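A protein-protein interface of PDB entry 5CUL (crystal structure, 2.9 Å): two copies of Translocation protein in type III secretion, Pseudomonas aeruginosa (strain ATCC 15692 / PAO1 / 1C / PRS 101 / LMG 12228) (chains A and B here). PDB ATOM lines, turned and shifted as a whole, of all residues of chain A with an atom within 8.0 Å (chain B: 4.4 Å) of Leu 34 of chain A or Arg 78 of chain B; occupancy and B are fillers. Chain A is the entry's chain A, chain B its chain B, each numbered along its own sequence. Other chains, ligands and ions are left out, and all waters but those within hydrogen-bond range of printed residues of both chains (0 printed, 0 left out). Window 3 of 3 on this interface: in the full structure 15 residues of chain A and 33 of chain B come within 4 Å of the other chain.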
ATOM      1  N   SER A  31      -4.120   1.608   2.133  1.00  0.00           N
ATOM      2  CA  SER A  31      -3.043   2.096   2.969  1.00  0.00           C
ATOM      3  C   SER A  31      -2.558   3.463   2.502  1.00  0.00           C
ATOM      4  O   SER A  31      -1.796   3.575   1.515  1.00  0.00           O
ATOM      5  CB  SER A  31      -1.922   1.119   2.882  1.00  0.00           C
ATOM      6  OG  SER A  31      -2.491  -0.185   2.766  1.00  0.00           O
ATOM      7  N   SER A  32      -3.001   4.496   3.226  1.00  0.00           N
ATOM      8  CA  SER A  32      -2.863   5.894   2.775  1.00  0.00           C
ATOM      9  C   SER A  32      -1.399   6.338   2.613  1.00  0.00           C
ATOM     10  O   SER A  32      -1.059   7.188   1.783  1.00  0.00           O
ATOM     11  CB  SER A  32      -3.647   6.848   3.726  1.00  0.00           C
ATOM     12  OG  SER A  32      -3.226   6.690   5.089  1.00  0.00           O
ATOM     13  N   ASN A  33      -0.529   5.748   3.405  1.00  0.00           N
ATOM     14  CA  ASN A  33       0.793   6.300   3.561  1.00  0.00           C
ATOM     15  C   ASN A  33       1.819   5.204   3.397  1.00  0.00           C
ATOM     16  O   ASN A  33       1.554   4.039   3.704  1.00  0.00           O
ATOM     17  CB  ASN A  33       0.887   6.979   4.958  1.00  0.00           C
ATOM     18  CG  ASN A  33       1.687   8.267   4.929  1.00  0.00           C
ATOM     19  OD1 ASN A  33       2.086   8.742   3.856  1.00  0.00           O
ATOM     20  ND2 ASN A  33       1.952   8.832   6.106  1.00  0.00           N
ATOM     21  N   LEU A  34       2.993   5.560   2.900  1.00  0.00           N
ATOM     22  CA  LEU A  34       4.111   4.644   3.002  1.00  0.00           C
ATOM     23  C   LEU A  34       4.467   4.495   4.482  1.00  0.00           C
ATOM     24  O   LEU A  34       4.699   3.383   4.972  1.00  0.00           O
ATOM     25  CB  LEU A  34       5.310   5.151   2.203  1.00  0.00           C
ATOM     26  CG  LEU A  34       6.559   4.241   2.317  1.00  0.00           C
ATOM     27  CD1 LEU A  34       6.313   2.816   1.825  1.00  0.00           C
ATOM     28  CD2 LEU A  34       7.728   4.847   1.577  1.00  0.00           C
ATOM     29  N   ARG A  35       4.490   5.634   5.182  1.00  0.00           N
ATOM     30  CA  ARG A  35       4.723   5.678   6.640  1.00  0.00           C
ATOM     31  C   ARG A  35       3.769   4.787   7.422  1.00  0.00           C
ATOM     32  O   ARG A  35       4.127   4.190   8.422  1.00  0.00           O
ATOM     33  CB  ARG A  35       4.598   7.112   7.129  1.00  0.00           C
ATOM     34  CG  ARG A  35       4.742   7.293   8.621  1.00  0.00           C
ATOM     35  CD  ARG A  35       4.823   8.767   8.960  1.00  0.00           C
ATOM     36  NE  ARG A  35       5.952   9.416   8.282  1.00  0.00           N
ATOM     37  CZ  ARG A  35       7.189   9.519   8.769  1.00  0.00           C
ATOM     38  NH1 ARG A  35       7.497   9.031   9.958  1.00  0.00           N
ATOM     39  NH2 ARG A  35       8.130  10.124   8.056  1.00  0.00           N
ATOM     40  N   ALA A  36       2.547   4.702   6.940  1.00  0.00           N
ATOM     41  CA  ALA A  36       1.555   3.866   7.547  1.00  0.00           C
ATOM     42  C   ALA A  36       2.020   2.425   7.546  1.00  0.00           C
ATOM     43  O   ALA A  36       1.927   1.741   8.570  1.00  0.00           O
ATOM     44  CB  ALA A  36       0.220   4.021   6.827  1.00  0.00           C
ATOM     45  N   ASP A  37       2.542   1.980   6.402  1.00  0.00           N
ATOM     46  CA  ASP A  37       2.998   0.583   6.217  1.00  0.00           C
ATOM     47  C   ASP A  37       4.227   0.309   7.044  1.00  0.00           C
ATOM     48  O   ASP A  37       4.340  -0.759   7.633  1.00  0.00           O
ATOM     49  CB  ASP A  37       3.293   0.294   4.744  1.00  0.00           C
ATOM     50  CG  ASP A  37       2.082   0.533   3.845  1.00  0.00           C
ATOM     51  OD1 ASP A  37       0.972   0.139   4.285  1.00  0.00           O
ATOM     52  OD2 ASP A  37       2.241   1.119   2.733  1.00  0.00           O
ATOM     53  N   VAL A  38       5.123   1.297   7.093  1.00  0.00           N
ATOM     54  CA  VAL A  38       6.339   1.225   7.905  1.00  0.00           C
ATOM     55  C   VAL A  38       5.992   1.112   9.380  1.00  0.00           C
ATOM     56  O   VAL A  38       6.634   0.397  10.130  1.00  0.00           O
ATOM     57  CB  VAL A  38       7.274   2.456   7.682  1.00  0.00           C
ATOM     58  CG1 VAL A  38       8.547   2.337   8.510  1.00  0.00           C
ATOM     59  CG2 VAL A  38       7.667   2.601   6.210  1.00  0.00           C
ATOM     60  N   ARG A  39       4.955   1.818   9.785  1.00  0.00           N
ATOM     61  CA  ARG A  39       4.498   1.787  11.167  1.00  0.00           C
ATOM     62  C   ARG A  39       3.773   0.502  11.531  1.00  0.00           C
ATOM     63  O   ARG A  39       3.816   0.085  12.676  1.00  0.00           O
ATOM     64  CB  ARG A  39       3.583   2.963  11.419  1.00  0.00           C
ATOM     65  CG  ARG A  39       4.342   4.273  11.548  1.00  0.00           C
ATOM     66  CD  ARG A  39       3.405   5.477  11.426  1.00  0.00           C
ATOM     67  NE  ARG A  39       2.360   5.499  12.463  1.00  0.00           N
ATOM     68  CZ  ARG A  39       2.552   5.848  13.742  1.00  0.00           C
ATOM     69  NH1 ARG A  39       3.748   6.218  14.188  1.00  0.00           N
ATOM     70  NH2 ARG A  39       1.536   5.818  14.595  1.00  0.00           N
ATOM     71  N   ARG A  40       3.109  -0.124  10.565  1.00  0.00           N
ATOM     72  CA  ARG A  40       2.548  -1.467  10.763  1.00  0.00           C
ATOM     73  C   ARG A  40       3.618  -2.524  11.129  1.00  0.00           C
ATOM     74  O   ARG A  40       3.300  -3.560  11.733  1.00  0.00           O
ATOM     75  CB  ARG A  40       1.857  -1.932   9.488  1.00  0.00           C
ATOM     76  CG  ARG A  40       0.538  -1.256   9.189  1.00  0.00           C
ATOM     77  CD  ARG A  40      -0.013  -1.743   7.848  1.00  0.00           C
ATOM     78  NE  ARG A  40      -0.212  -3.205   7.837  1.00  0.00           N
ATOM     79  CZ  ARG A  40      -0.228  -3.975   6.739  1.00  0.00           C
ATOM     80  NH1 ARG A  40      -0.046  -3.440   5.521  1.00  0.00           N
ATOM     81  NH2 ARG A  40      -0.417  -5.293   6.855  1.00  0.00           N
ATOM     82  N   SER A  41       4.874  -2.254  10.747  1.00  0.00           N
ATOM     83  CA  SER A  41       5.951  -3.238  10.802  1.00  0.00           C
ATOM     84  C   SER A  41       6.578  -3.379  12.184  1.00  0.00           C
ATOM     85  O   SER A  41       6.677  -2.420  12.939  1.00  0.00           O
ATOM     86  CB  SER A  41       7.043  -2.890   9.782  1.00  0.00           C
ATOM     87  OG  SER A  41       6.507  -2.668   8.484  1.00  0.00           O
ATOM     88  N   HIS B  71       9.995  -3.102  -0.904  1.00  0.00           N
ATOM     89  CA  HIS B  71      10.483  -1.972  -1.709  1.00  0.00           C
ATOM     90  C   HIS B  71      11.939  -2.139  -2.067  1.00  0.00           C
ATOM     91  O   HIS B  71      12.700  -2.720  -1.313  1.00  0.00           O
ATOM     92  CB  HIS B  71      10.255  -0.621  -1.008  1.00  0.00           C
ATOM     93  CG  HIS B  71       8.817  -0.186  -0.985  1.00  0.00           C
ATOM     94  ND1 HIS B  71       8.139   0.201  -2.122  1.00  0.00           N
ATOM     95  CD2 HIS B  71       7.926  -0.095   0.034  1.00  0.00           C
ATOM     96  CE1 HIS B  71       6.891   0.509  -1.803  1.00  0.00           C
ATOM     97  NE2 HIS B  71       6.732   0.327  -0.502  1.00  0.00           N
ATOM     98  N   ALA B  74      15.212   3.407  -4.383  1.00  0.00           N
ATOM     99  CA  ALA B  74      14.930   4.669  -3.697  1.00  0.00           C
ATOM    100  C   ALA B  74      13.855   4.508  -2.616  1.00  0.00           C
ATOM    101  O   ALA B  74      14.005   5.024  -1.523  1.00  0.00           O
ATOM    102  CB  ALA B  74      14.512   5.714  -4.714  1.00  0.00           C
ATOM    103  N   LEU B  75      12.782   3.788  -2.934  1.00  0.00           N
ATOM    104  CA  LEU B  75      11.710   3.553  -1.976  1.00  0.00           C
ATOM    105  C   LEU B  75      12.170   2.707  -0.800  1.00  0.00           C
ATOM    106  O   LEU B  75      11.672   2.880   0.322  1.00  0.00           O
ATOM    107  CB  LEU B  75      10.515   2.895  -2.652  1.00  0.00           C
ATOM    108  CG  LEU B  75       9.635   3.851  -3.450  1.00  0.00           C
ATOM    109  CD1 LEU B  75       8.386   3.125  -3.967  1.00  0.00           C
ATOM    110  CD2 LEU B  75       9.247   5.075  -2.618  1.00  0.00           C
ATOM    111  N   ALA B  76      13.113   1.801  -1.061  1.00  0.00           N
ATOM    112  CA  ALA B  76      13.712   0.990   0.001  1.00  0.00           C
ATOM    113  C   ALA B  76      14.475   1.851   0.994  1.00  0.00           C
ATOM    114  O   ALA B  76      14.421   1.630   2.187  1.00  0.00           O
ATOM    115  CB  ALA B  76      14.631  -0.059  -0.579  1.00  0.00           C
ATOM    116  N   LEU B  77      15.173   2.852   0.494  1.00  0.00           N
ATOM    117  CA  LEU B  77      15.872   3.810   1.353  1.00  0.00           C
ATOM    118  C   LEU B  77      14.926   4.758   2.109  1.00  0.00           C
ATOM    119  O   LEU B  77      15.192   5.172   3.246  1.00  0.00           O
ATOM    120  CB  LEU B  77      16.854   4.615   0.490  1.00  0.00           C
ATOM    121  CG  LEU B  77      18.047   3.819  -0.043  1.00  0.00           C
ATOM    122  CD1 LEU B  77      18.920   4.729  -0.896  1.00  0.00           C
ATOM    123  CD2 LEU B  77      18.873   3.199   1.093  1.00  0.00           C
ATOM    124  N   ARG B  78      13.825   5.104   1.443  1.00  0.00           N
ATOM    125  CA  ARG B  78      12.783   5.929   2.048  1.00  0.00           C
ATOM    126  C   ARG B  78      12.149   5.200   3.206  1.00  0.00           C
ATOM    127  O   ARG B  78      11.891   5.784   4.235  1.00  0.00           O
ATOM    128  CB  ARG B  78      11.703   6.294   1.031  1.00  0.00           C
ATOM    129  CG  ARG B  78      10.640   7.235   1.593  1.00  0.00           C
ATOM    130  CD  ARG B  78      11.222   8.617   1.900  1.00  0.00           C
ATOM    131  NE  ARG B  78      10.492   9.317   2.958  1.00  0.00           N
ATOM    132  CZ  ARG B  78      11.036  10.210   3.791  1.00  0.00           C
ATOM    133  NH1 ARG B  78      12.328  10.529   3.709  1.00  0.00           N
ATOM    134  NH2 ARG B  78      10.289  10.791   4.723  1.00  0.00           N
ATOM    135  N   VAL B  79      11.929   3.912   3.012  1.00  0.00           N
ATOM    136  CA  VAL B  79      11.434   3.041   4.064  1.00  0.00           C
ATOM    137  C   VAL B  79      12.336   3.029   5.273  1.00  0.00           C
ATOM    138  O   VAL B  79      11.872   3.063   6.391  1.00  0.00           O
ATOM    139  CB  VAL B  79      11.267   1.593   3.551  1.00  0.00           C
ATOM    140  CG1 VAL B  79      11.150   0.624   4.712  1.00  0.00           C
ATOM    141  CG2 VAL B  79      10.033   1.480   2.647  1.00  0.00           C
ATOM    142  N   ARG B  80      13.630   2.973   5.037  1.00  0.00           N
ATOM    143  CA  ARG B  80      14.609   2.930   6.128  1.00  0.00           C
ATOM    144  C   ARG B  80      14.668   4.215   6.891  1.00  0.00           C
ATOM    145  O   ARG B  80      14.807   4.209   8.098  1.00  0.00           O
ATOM    146  CB  ARG B  80      16.002   2.580   5.611  1.00  0.00           C
ATOM    147  CG  ARG B  80      16.172   1.078   5.359  1.00  0.00           C
ATOM    148  CD  ARG B  80      17.208   0.772   4.279  1.00  0.00           C
ATOM    149  NE  ARG B  80      18.597   0.831   4.763  1.00  0.00           N
ATOM    150  CZ  ARG B  80      19.643   0.306   4.116  1.00  0.00           C
ATOM    151  NH1 ARG B  80      19.479  -0.334   2.947  1.00  0.00           N
ATOM    152  NH2 ARG B  80      20.863   0.410   4.641  1.00  0.00           N
ATOM    153  N   ARG B  81      14.564   5.322   6.193  1.00  0.00           N
ATOM    154  CA  ARG B  81      14.562   6.597   6.866  1.00  0.00           C
ATOM    155  C   ARG B  81      13.290   6.804   7.674  1.00  0.00           C
ATOM    156  O   ARG B  81      13.328   7.318   8.761  1.00  0.00           O
ATOM    157  CB  ARG B  81      14.735   7.727   5.863  1.00  0.00           C
ATOM    158  CG  ARG B  81      15.107   9.050   6.526  1.00  0.00           C
ATOM    159  CD  ARG B  81      14.968  10.209   5.553  1.00  0.00           C
ATOM    160  NE  ARG B  81      16.040  11.198   5.704  1.00  0.00           N
ATOM    161  CZ  ARG B  81      16.180  12.287   4.941  1.00  0.00           C
ATOM    162  NH1 ARG B  81      15.313  12.542   3.964  1.00  0.00           N
ATOM    163  NH2 ARG B  81      17.196  13.128   5.149  1.00  0.00           N
ATOM    164  N   ILE B  82      12.164   6.406   7.133  1.00  0.00           N
ATOM    165  CA  ILE B  82      10.912   6.477   7.856  1.00  0.00           C
ATOM    166  C   ILE B  82      10.938   5.579   9.084  1.00  0.00           C
ATOM    167  O   ILE B  82      10.412   5.937  10.129  1.00  0.00           O
ATOM    168  CB  ILE B  82       9.748   6.056   6.943  1.00  0.00           C
ATOM    169  CG1 ILE B  82       9.556   7.091   5.838  1.00  0.00           C
ATOM    170  CG2 ILE B  82       8.455   5.905   7.733  1.00  0.00           C
ATOM    171  CD1 ILE B  82       8.406   6.783   4.900  1.00  0.00           C
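The backbone carbonyl oxygen (O) of Val 38 of chain A sits close to the side-chain hydroxyl (OG) of Ser 41 of chain A (3.5 Å).
CD1 of Leu 34 of chain A touches NE2 of His 71 of chain B, at 3.4 Å. Leu 34 of chain A touches Arg 78 of chain B (CD2 to CG, 3.8 Å). Ile 82 of chain B touches Leu 34 of chain A. CA of Arg 35 of chain A touches CG2 of Ile 82 of chain B, 3.9 Å away. Val 38 of chain A touches Ile 82 of chain B (CB to CG2, 3.6 Å).
Asn 33 of chain A touches none of the printed residues of chain B. Leu 34 of chain A touches just these residues of chain B: His 71, Arg 78 and Ile 82. Printed residues of chain B within 4 Å of Arg 35 of chain A: Ile 82. Printed residues of chain B within 4 Å of Val 38 of chain A: Ile 82. Of the printed residues of chain A, His 71 of chain B touches Leu 34. Of the printed residues of chain A, Ile 82 of chain B touches Leu 34 (3.9 Å), Arg 35 (3.9 Å) and Val 38 (3.6 Å). The nearest residue of chain A that does not touch Arg 78 of chain B is Arg 35 of chain A (4.03 Å).
Of the 10 printed residues of chain B, 3 touch a printed residue of chain A. Hydrophobic or aromatic side chains of chain B within 4 Å of the printed part of chain A: His 71 and Ile 82.
No position is printed for both chains. Of the 5 pairs that touch across the chains among the printed residues, none has its exchanged pair printed and touching as well.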
